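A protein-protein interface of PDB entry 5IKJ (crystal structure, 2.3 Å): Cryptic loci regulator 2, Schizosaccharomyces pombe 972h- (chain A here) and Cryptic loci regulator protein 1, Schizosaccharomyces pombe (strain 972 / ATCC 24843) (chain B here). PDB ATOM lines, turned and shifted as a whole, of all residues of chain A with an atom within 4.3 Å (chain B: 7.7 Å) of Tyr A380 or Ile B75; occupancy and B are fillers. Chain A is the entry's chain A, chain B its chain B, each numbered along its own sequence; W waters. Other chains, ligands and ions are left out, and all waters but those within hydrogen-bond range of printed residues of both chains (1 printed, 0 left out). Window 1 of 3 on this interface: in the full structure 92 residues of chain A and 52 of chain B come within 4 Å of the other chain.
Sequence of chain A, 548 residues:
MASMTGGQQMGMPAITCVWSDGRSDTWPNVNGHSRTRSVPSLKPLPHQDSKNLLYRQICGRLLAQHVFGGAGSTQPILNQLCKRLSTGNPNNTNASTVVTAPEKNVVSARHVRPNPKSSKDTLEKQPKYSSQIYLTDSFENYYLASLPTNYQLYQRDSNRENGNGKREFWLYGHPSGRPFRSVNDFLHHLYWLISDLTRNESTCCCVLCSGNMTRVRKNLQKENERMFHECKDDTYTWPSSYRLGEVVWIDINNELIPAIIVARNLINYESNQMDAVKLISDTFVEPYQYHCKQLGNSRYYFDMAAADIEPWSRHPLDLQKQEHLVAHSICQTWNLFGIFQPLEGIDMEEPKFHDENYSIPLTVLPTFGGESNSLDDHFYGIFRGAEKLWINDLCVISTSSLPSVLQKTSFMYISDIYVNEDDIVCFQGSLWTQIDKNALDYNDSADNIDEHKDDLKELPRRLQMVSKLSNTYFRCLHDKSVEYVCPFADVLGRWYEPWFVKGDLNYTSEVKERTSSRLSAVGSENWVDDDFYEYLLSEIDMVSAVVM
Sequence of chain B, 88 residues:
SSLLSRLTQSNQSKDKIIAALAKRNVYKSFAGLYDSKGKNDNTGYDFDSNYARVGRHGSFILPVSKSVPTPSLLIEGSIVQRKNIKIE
Water W1 lies within hydrogen-bond range of NZ of Lys A232, O of Leu B74, O of Ile B75 and N of Gly B77.
NZ of Lys A232 lies within hydrogen-bond range of O of Glu B76, 3.4 Å away. O of Ser B72 lies close to OD1 of Asn A392 (3.3 Å). The side-chain amino group (NZ) of Lys A232 lies within hydrogen-bond range of the backbone carbonyl oxygen (O) of Ile B75 (2.9 Å). ND2 of Asn A392 lies within hydrogen-bond range of OE1 of Glu B76 (3.1 Å).
Tyr A380 touches one residue of chain B. Of the printed residues of chain A, Ile B75 touches Phe A228 (3.6 Å), Cys A231 (3.6 Å), Lys A232 (2.9 Å), Thr A235 (3.6 Å), Tyr A380 (3.7 Å) and Ile A391 (3.8 Å). Of the printed residues of chain B, Ile A391 touches Pro B71 and Ile B75. Printed residues of chain B within 4 Å of Thr A235: Ile B75 (3.6 Å). Of the printed residues of chain B, Lys A232 touches Ile B75 (2.9 Å) and Glu B76 (3.4 Å). Printed residues of chain B within 4 Å of Trp A390: Ala B31 (3.5 Å). Of the printed residues of chain B, Phe A340 touches Pro B71 (3.5 Å). Ile B79 touches none of the printed residues of chain A. Gly A381 touches none of the printed residues of chain B. The nearest residue of chain B that does not touch Tyr A380 is Ala B31 (6.4 Å). The nearest printed residue of chain A that does not touch Ile B75 is Asn A392 (4.01 Å). The nearest printed residue of chain B that does not touch Lys A232 is Gly B77 (4.1 Å).
Among the printed residues, merely in contact across the chains: Met A227 with Ala B31, Phe A228 with Leu B74, Phe A228 with Ile B75, Cys A231 with Ile B75, Thr A235 with Ile B75, Phe A337 with Ala B31, Phe A340 with Pro B71, Phe A368 with Leu B74, Tyr A380 with Ile B75, Trp A390 with Ala B31, Ile A391 with Pro B71 and Ile A391 with Ile B75.
Printed residues of chain A that touch a printed residue of chain B: Met A227, Phe A228, Cys A231, Lys A232, Thr A235, Phe A337, Phe A340, Phe A368, Tyr A380, Trp A390, Ile A391 and Asn A392. Hydrophobic or aromatic side chains of chain A within 4 Å of the printed part of chain B: Met A227, Phe A228, Phe A337, Phe A340, Phe A368, Tyr A380, Trp A390 and Ile A391. Printed residues of chain B that touch a printed residue of chain A: Ala B31, Pro B71, Ser B72, Leu B74, Ile B75 and Glu B76. Among the printed residues, no Asp or Glu carboxylate lies within 4 Å of a Lys or Arg side-chain nitrogen of the other chain.
The side-chain hydroxyl of Thr A235 lies within hydrogen-bond range of the backbone carbonyl oxygen of Cys A231, 3.0 Å away. N of Tyr A380 sits at hydrogen-bond distance from O of Gly A338 (2.7 Å). The backbone carbonyl oxygen (O) of Phe A337 lies within hydrogen-bond range of the backbone NH (N) of Tyr A380. The side-chain sulfur of Cys A231 sits at hydrogen-bond distance from the backbone carbonyl oxygen of Ile A391 (3.5 Å). OG of Ser B72 sits at hydrogen-bond distance from OG1 of Thr B70 (3.0 Å). The side-chain hydroxyl of Thr A235 is in hydrogen-bond range of the side-chain amide nitrogen of Asn A392 (3.0 Å).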
ATOM      1  N   MET A 227      16.180  -3.785 -15.506  1.00  0.00           N
ATOM      2  CA  MET A 227      17.457  -3.113 -15.329  1.00  0.00           C
ATOM      3  C   MET A 227      17.436  -2.295 -14.051  1.00  0.00           C
ATOM      4  O   MET A 227      18.386  -2.312 -13.288  1.00  0.00           O
ATOM      5  CB  MET A 227      17.786  -2.212 -16.504  1.00  0.00           C
ATOM      6  CG  MET A 227      19.116  -1.507 -16.344  1.00  0.00           C
ATOM      7  SD  MET A 227      19.585  -0.603 -17.808  1.00  0.00           S
ATOM      8  CE  MET A 227      18.200   0.503 -17.961  1.00  0.00           C
ATOM      9  N   PHE A 228      16.347  -1.578 -13.822  1.00  0.00           N
ATOM     10  CA  PHE A 228      16.220  -0.784 -12.604  1.00  0.00           C
ATOM     11  C   PHE A 228      16.417  -1.651 -11.369  1.00  0.00           C
ATOM     12  O   PHE A 228      17.156  -1.286 -10.447  1.00  0.00           O
ATOM     13  CB  PHE A 228      14.853  -0.100 -12.562  1.00  0.00           C
ATOM     14  CG  PHE A 228      14.501   0.466 -11.216  1.00  0.00           C
ATOM     15  CD1 PHE A 228      14.971   1.709 -10.826  1.00  0.00           C
ATOM     16  CD2 PHE A 228      13.699  -0.247 -10.337  1.00  0.00           C
ATOM     17  CE1 PHE A 228      14.652   2.229  -9.588  1.00  0.00           C
ATOM     18  CE2 PHE A 228      13.377   0.270  -9.097  1.00  0.00           C
ATOM     19  CZ  PHE A 228      13.853   1.510  -8.722  1.00  0.00           C
ATOM     20  N   CYS A 231      19.912  -2.836 -10.969  1.00  0.00           N
ATOM     21  CA  CYS A 231      20.681  -1.743 -10.387  1.00  0.00           C
ATOM     22  C   CYS A 231      20.431  -1.640  -8.889  1.00  0.00           C
ATOM     23  O   CYS A 231      21.371  -1.603  -8.087  1.00  0.00           O
ATOM     24  CB  CYS A 231      20.305  -0.438 -11.088  1.00  0.00           C
ATOM     25  SG  CYS A 231      21.234   0.990 -10.550  1.00  0.00           S
ATOM     26  N   LYS A 232      19.159  -1.593  -8.496  1.00  0.00           N
ATOM     27  CA  LYS A 232      18.814  -1.482  -7.084  1.00  0.00           C
ATOM     28  C   LYS A 232      19.415  -2.629  -6.281  1.00  0.00           C
ATOM     29  O   LYS A 232      19.923  -2.422  -5.173  1.00  0.00           O
ATOM     30  CB  LYS A 232      17.295  -1.452  -6.929  1.00  0.00           C
ATOM     31  CG  LYS A 232      16.806  -0.995  -5.566  1.00  0.00           C
ATOM     32  CD  LYS A 232      15.289  -0.872  -5.549  1.00  0.00           C
ATOM     33  CE  LYS A 232      14.755  -0.538  -4.164  1.00  0.00           C
ATOM     34  NZ  LYS A 232      15.149   0.825  -3.707  1.00  0.00           N
ATOM     35  N   THR A 235      23.228  -2.260  -5.777  1.00  0.00           N
ATOM     36  CA  THR A 235      23.660  -1.119  -4.982  1.00  0.00           C
ATOM     37  C   THR A 235      22.863  -0.911  -3.701  1.00  0.00           C
ATOM     38  O   THR A 235      23.313  -0.142  -2.845  1.00  0.00           O
ATOM     39  CB  THR A 235      23.585   0.174  -5.810  1.00  0.00           C
ATOM     40  OG1 THR A 235      22.220   0.465  -6.129  1.00  0.00           O
ATOM     41  CG2 THR A 235      24.386   0.040  -7.099  1.00  0.00           C
ATOM     42  N   PHE A 337      25.656   1.117 -20.938  1.00  0.00           N
ATOM     43  CA  PHE A 337      24.349   0.510 -21.133  1.00  0.00           C
ATOM     44  C   PHE A 337      23.321   1.239 -20.279  1.00  0.00           C
ATOM     45  O   PHE A 337      23.655   1.892 -19.289  1.00  0.00           O
ATOM     46  CB  PHE A 337      24.359  -0.986 -20.784  1.00  0.00           C
ATOM     47  CG  PHE A 337      24.828  -1.282 -19.388  1.00  0.00           C
ATOM     48  CD1 PHE A 337      23.950  -1.223 -18.319  1.00  0.00           C
ATOM     49  CD2 PHE A 337      26.145  -1.630 -19.148  1.00  0.00           C
ATOM     50  CE1 PHE A 337      24.379  -1.497 -17.035  1.00  0.00           C
ATOM     51  CE2 PHE A 337      26.581  -1.908 -17.866  1.00  0.00           C
ATOM     52  CZ  PHE A 337      25.696  -1.841 -16.808  1.00  0.00           C
ATOM     53  N   GLY A 338      22.060   1.119 -20.684  1.00  0.00           N
ATOM     54  CA  GLY A 338      20.958   1.641 -19.901  1.00  0.00           C
ATOM     55  C   GLY A 338      20.793   3.143 -19.986  1.00  0.00           C
ATOM     56  O   GLY A 338      20.777   3.830 -18.960  1.00  0.00           O
ATOM     57  N   PHE A 340      18.986   6.644 -20.202  1.00  0.00           N
ATOM     58  CA  PHE A 340      17.733   7.112 -19.632  1.00  0.00           C
ATOM     59  C   PHE A 340      17.748   8.632 -19.582  1.00  0.00           C
ATOM     60  O   PHE A 340      18.784   9.274 -19.767  1.00  0.00           O
ATOM     61  CB  PHE A 340      17.503   6.531 -18.232  1.00  0.00           C
ATOM     62  CG  PHE A 340      18.402   7.111 -17.182  1.00  0.00           C
ATOM     63  CD1 PHE A 340      19.715   6.693 -17.071  1.00  0.00           C
ATOM     64  CD2 PHE A 340      17.932   8.073 -16.304  1.00  0.00           C
ATOM     65  CE1 PHE A 340      20.546   7.223 -16.104  1.00  0.00           C
ATOM     66  CE2 PHE A 340      18.760   8.611 -15.335  1.00  0.00           C
ATOM     67  CZ  PHE A 340      20.066   8.186 -15.235  1.00  0.00           C
ATOM     68  N   PHE A 368      11.651   6.471 -16.937  1.00  0.00           N
ATOM     69  CA  PHE A 368      12.565   7.513 -17.396  1.00  0.00           C
ATOM     70  C   PHE A 368      12.253   7.944 -18.823  1.00  0.00           C
ATOM     71  O   PHE A 368      12.389   9.125 -19.162  1.00  0.00           O
ATOM     72  CB  PHE A 368      14.009   7.025 -17.300  1.00  0.00           C
ATOM     73  CG  PHE A 368      14.546   6.979 -15.901  1.00  0.00           C
ATOM     74  CD1 PHE A 368      14.472   8.092 -15.080  1.00  0.00           C
ATOM     75  CD2 PHE A 368      15.148   5.829 -15.413  1.00  0.00           C
ATOM     76  CE1 PHE A 368      14.973   8.053 -13.795  1.00  0.00           C
ATOM     77  CE2 PHE A 368      15.651   5.785 -14.129  1.00  0.00           C
ATOM     78  CZ  PHE A 368      15.563   6.898 -13.318  1.00  0.00           C
ATOM     79  N   PHE A 379      23.474   7.282 -18.331  1.00  0.00           N
ATOM     80  CA  PHE A 379      23.487   5.831 -18.439  1.00  0.00           C
ATOM     81  C   PHE A 379      23.412   5.190 -17.062  1.00  0.00           C
ATOM     82  O   PHE A 379      24.041   5.657 -16.109  1.00  0.00           O
ATOM     83  CB  PHE A 379      24.748   5.351 -19.169  1.00  0.00           C
ATOM     84  CG  PHE A 379      24.793   5.747 -20.614  1.00  0.00           C
ATOM     85  CD1 PHE A 379      24.229   4.938 -21.584  1.00  0.00           C
ATOM     86  CD2 PHE A 379      25.392   6.933 -21.003  1.00  0.00           C
ATOM     87  CE1 PHE A 379      24.263   5.300 -22.915  1.00  0.00           C
ATOM     88  CE2 PHE A 379      25.430   7.302 -22.335  1.00  0.00           C
ATOM     89  CZ  PHE A 379      24.865   6.482 -23.291  1.00  0.00           C
ATOM     90  N   TYR A 380      22.641   4.103 -16.978  1.00  0.00           N
ATOM     91  CA  TYR A 380      22.509   3.366 -15.725  1.00  0.00           C
ATOM     92  C   TYR A 380      23.852   2.836 -15.242  1.00  0.00           C
ATOM     93  O   TYR A 380      24.125   2.825 -14.035  1.00  0.00           O
ATOM     94  CB  TYR A 380      21.536   2.204 -15.909  1.00  0.00           C
ATOM     95  CG  TYR A 380      20.176   2.413 -15.304  1.00  0.00           C
ATOM     96  CD1 TYR A 380      19.182   3.092 -15.992  1.00  0.00           C
ATOM     97  CD2 TYR A 380      19.877   1.908 -14.051  1.00  0.00           C
ATOM     98  CE1 TYR A 380      17.930   3.269 -15.439  1.00  0.00           C
ATOM     99  CE2 TYR A 380      18.637   2.081 -13.492  1.00  0.00           C
ATOM    100  CZ  TYR A 380      17.664   2.761 -14.185  1.00  0.00           C
ATOM    101  OH  TYR A 380      16.424   2.920 -13.609  1.00  0.00           O
ATOM    102  N   GLY A 381      24.694   2.374 -16.158  1.00  0.00           N
ATOM    103  CA  GLY A 381      25.904   1.694 -15.739  1.00  0.00           C
ATOM    104  C   GLY A 381      26.871   1.514 -16.888  1.00  0.00           C
ATOM    105  O   GLY A 381      26.633   1.955 -18.014  1.00  0.00           O
ATOM    106  N   TRP A 390      27.580   0.836 -11.672  1.00  0.00           N
ATOM    107  CA  TRP A 390      26.244   1.406 -11.727  1.00  0.00           C
ATOM    108  C   TRP A 390      26.232   2.814 -11.149  1.00  0.00           C
ATOM    109  O   TRP A 390      27.162   3.244 -10.460  1.00  0.00           O
ATOM    110  CB  TRP A 390      25.235   0.571 -10.928  1.00  0.00           C
ATOM    111  CG  TRP A 390      24.980  -0.833 -11.413  1.00  0.00           C
ATOM    112  CD1 TRP A 390      25.618  -1.974 -11.003  1.00  0.00           C
ATOM    113  CD2 TRP A 390      23.988  -1.250 -12.362  1.00  0.00           C
ATOM    114  NE1 TRP A 390      25.092  -3.067 -11.647  1.00  0.00           N
ATOM    115  CE2 TRP A 390      24.092  -2.652 -12.487  1.00  0.00           C
ATOM    116  CE3 TRP A 390      23.027  -0.577 -13.122  1.00  0.00           C
ATOM    117  CZ2 TRP A 390      23.273  -3.388 -13.344  1.00  0.00           C
ATOM    118  CZ3 TRP A 390      22.216  -1.311 -13.972  1.00  0.00           C
ATOM    119  CH2 TRP A 390      22.344  -2.701 -14.075  1.00  0.00           C
ATOM    120  N   ILE A 391      25.142   3.525 -11.434  1.00  0.00           N
ATOM    121  CA  ILE A 391      24.763   4.667 -10.617  1.00  0.00           C
ATOM    122  C   ILE A 391      24.313   4.155  -9.252  1.00  0.00           C
ATOM    123  O   ILE A 391      23.737   3.065  -9.132  1.00  0.00           O
ATOM    124  CB  ILE A 391      23.656   5.495 -11.296  1.00  0.00           C
ATOM    125  CG1 ILE A 391      22.406   4.639 -11.531  1.00  0.00           C
ATOM    126  CG2 ILE A 391      24.167   6.079 -12.611  1.00  0.00           C
ATOM    127  CD1 ILE A 391      21.209   5.408 -12.066  1.00  0.00           C
ATOM    128  N   ASN A 392      24.587   4.939  -8.210  1.00  0.00           N
ATOM    129  CA  ASN A 392      24.306   4.583  -6.818  1.00  0.00           C
ATOM    130  C   ASN A 392      25.320   3.572  -6.301  1.00  0.00           C
ATOM    131  O   ASN A 392      25.154   3.046  -5.187  1.00  0.00           O
ATOM    132  CB  ASN A 392      22.891   4.020  -6.642  1.00  0.00           C
ATOM    133  CG  ASN A 392      22.385   4.135  -5.219  1.00  0.00           C
ATOM    134  OD1 ASN A 392      22.554   5.167  -4.569  1.00  0.00           O
ATOM    135  ND2 ASN A 392      21.761   3.070  -4.724  1.00  0.00           N
ATOM    136  N   ALA B  31      21.100  -6.352 -17.993  1.00  0.00           N
ATOM    137  CA  ALA B  31      21.583  -5.042 -18.409  1.00  0.00           C
ATOM    138  C   ALA B  31      22.985  -5.138 -18.999  1.00  0.00           C
ATOM    139  O   ALA B  31      23.894  -5.710 -18.388  1.00  0.00           O
ATOM    140  CB  ALA B  31      21.575  -4.082 -17.222  1.00  0.00           C
ATOM    141  N   THR B  70      19.813  13.488  -7.701  1.00  0.00           N
ATOM    142  CA  THR B  70      20.519  12.819  -8.779  1.00  0.00           C
ATOM    143  C   THR B  70      19.865  11.479  -9.098  1.00  0.00           C
ATOM    144  O   THR B  70      19.097  10.944  -8.293  1.00  0.00           O
ATOM    145  CB  THR B  70      21.981  12.606  -8.401  1.00  0.00           C
ATOM    146  OG1 THR B  70      22.058  11.987  -7.109  1.00  0.00           O
ATOM    147  CG2 THR B  70      22.727  13.932  -8.374  1.00  0.00           C
ATOM    148  N   PRO B  71      20.147  10.917 -10.277  1.00  0.00           N
ATOM    149  CA  PRO B  71      19.570   9.605 -10.616  1.00  0.00           C
ATOM    150  C   PRO B  71      19.773   8.549  -9.542  1.00  0.00           C
ATOM    151  O   PRO B  71      18.886   7.717  -9.320  1.00  0.00           O
ATOM    152  CB  PRO B  71      20.302   9.238 -11.913  1.00  0.00           C
ATOM    153  CG  PRO B  71      20.647  10.546 -12.528  1.00  0.00           C
ATOM    154  CD  PRO B  71      20.942  11.476 -11.385  1.00  0.00           C
ATOM    155  N   SER B  72      20.920   8.568  -8.859  1.00  0.00           N
ATOM    156  CA  SER B  72      21.235   7.517  -7.897  1.00  0.00           C
ATOM    157  C   SER B  72      20.178   7.400  -6.806  1.00  0.00           C
ATOM    158  O   SER B  72      19.941   6.302  -6.292  1.00  0.00           O
ATOM    159  CB  SER B  72      22.602   7.783  -7.272  1.00  0.00           C
ATOM    160  OG  SER B  72      22.628   9.047  -6.631  1.00  0.00           O
ATOM    161  N   LEU B  73      19.537   8.510  -6.435  1.00  0.00           N
ATOM    162  CA  LEU B  73      18.611   8.493  -5.311  1.00  0.00           C
ATOM    163  C   LEU B  73      17.279   7.837  -5.652  1.00  0.00           C
ATOM    164  O   LEU B  73      16.592   7.363  -4.742  1.00  0.00           O
ATOM    165  CB  LEU B  73      18.374   9.917  -4.800  1.00  0.00           C
ATOM    166  CG  LEU B  73      19.580  10.634  -4.186  1.00  0.00           C
ATOM    167  CD1 LEU B  73      19.158  11.996  -3.659  1.00  0.00           C
ATOM    168  CD2 LEU B  73      20.230   9.815  -3.075  1.00  0.00           C
ATOM    169  N   LEU B  74      16.896   7.801  -6.930  1.00  0.00           N
ATOM    170  CA  LEU B  74      15.730   7.013  -7.319  1.00  0.00           C
ATOM    171  C   LEU B  74      16.008   5.523  -7.183  1.00  0.00           C
ATOM    172  O   LEU B  74      15.086   4.743  -6.919  1.00  0.00           O
ATOM    173  CB  LEU B  74      15.319   7.347  -8.752  1.00  0.00           C
ATOM    174  CG  LEU B  74      14.758   8.751  -8.980  1.00  0.00           C
ATOM    175  CD1 LEU B  74      14.902   9.142 -10.441  1.00  0.00           C
ATOM    176  CD2 LEU B  74      13.300   8.830  -8.543  1.00  0.00           C
ATOM    177  N   ILE B  75      17.266   5.114  -7.359  1.00  0.00           N
ATOM    178  CA  ILE B  75      17.638   3.720  -7.140  1.00  0.00           C
ATOM    179  C   ILE B  75      17.607   3.398  -5.652  1.00  0.00           C
ATOM    180  O   ILE B  75      17.145   2.326  -5.243  1.00  0.00           O
ATOM    181  CB  ILE B  75      19.027   3.436  -7.742  1.00  0.00           C
ATOM    182  CG1 ILE B  75      19.131   3.964  -9.177  1.00  0.00           C
ATOM    183  CG2 ILE B  75      19.325   1.945  -7.699  1.00  0.00           C
ATOM    184  CD1 ILE B  75      18.090   3.414 -10.135  1.00  0.00           C
ATOM    185  N   GLU B  76      18.098   4.319  -4.820  1.00  0.00           N
ATOM    186  CA  GLU B  76      18.149   4.083  -3.383  1.00  0.00           C
ATOM    187  C   GLU B  76      16.757   4.043  -2.769  1.00  0.00           C
ATOM    188  O   GLU B  76      16.531   3.318  -1.795  1.00  0.00           O
ATOM    189  CB  GLU B  76      18.992   5.169  -2.711  1.00  0.00           C
ATOM    190  CG  GLU B  76      19.176   5.007  -1.206  1.00  0.00           C
ATOM    191  CD  GLU B  76      20.219   3.970  -0.845  1.00  0.00           C
ATOM    192  OE1 GLU B  76      20.920   3.486  -1.756  1.00  0.00           O
ATOM    193  OE2 GLU B  76      20.342   3.645   0.355  1.00  0.00           O
ATOM    194  N   GLY B  77      15.815   4.807  -3.320  1.00  0.00           N
ATOM    195  CA  GLY B  77      14.488   4.929  -2.758  1.00  0.00           C
ATOM    196  C   GLY B  77      14.299   6.133  -1.862  1.00  0.00           C
ATOM    197  O   GLY B  77      13.161   6.412  -1.465  1.00  0.00           O
ATOM    198  N   SER B  78      15.377   6.849  -1.530  1.00  0.00           N
ATOM    199  CA  SER B  78      15.250   8.061  -0.728  1.00  0.00           C
ATOM    200  C   SER B  78      14.301   9.056  -1.378  1.00  0.00           C
ATOM    201  O   SER B  78      13.683   9.872  -0.685  1.00  0.00           O
ATOM    202  CB  SER B  78      16.624   8.701  -0.530  1.00  0.00           C
ATOM    203  OG  SER B  78      17.564   7.750  -0.067  1.00  0.00           O
ATOM    204  N   ILE B  79      14.171   9.003  -2.701  1.00  0.00           N
ATOM    205  CA  ILE B  79      13.306   9.904  -3.448  1.00  0.00           C
ATOM    206  C   ILE B  79      12.619   9.097  -4.538  1.00  0.00           C
ATOM    207  O   ILE B  79      13.202   8.173  -5.114  1.00  0.00           O
ATOM    208  CB  ILE B  79      14.101  11.098  -4.030  1.00  0.00           C
ATOM    209  CG1 ILE B  79      14.283  12.164  -2.942  1.00  0.00           C
ATOM    210  CG2 ILE B  79      13.418  11.678  -5.275  1.00  0.00           C
ATOM    211  CD1 ILE B  79      15.158  13.327  -3.341  1.00  0.00           C
HETATM  212  O   HOH W   1      13.883   2.727  -5.250  1.00  0.00           O
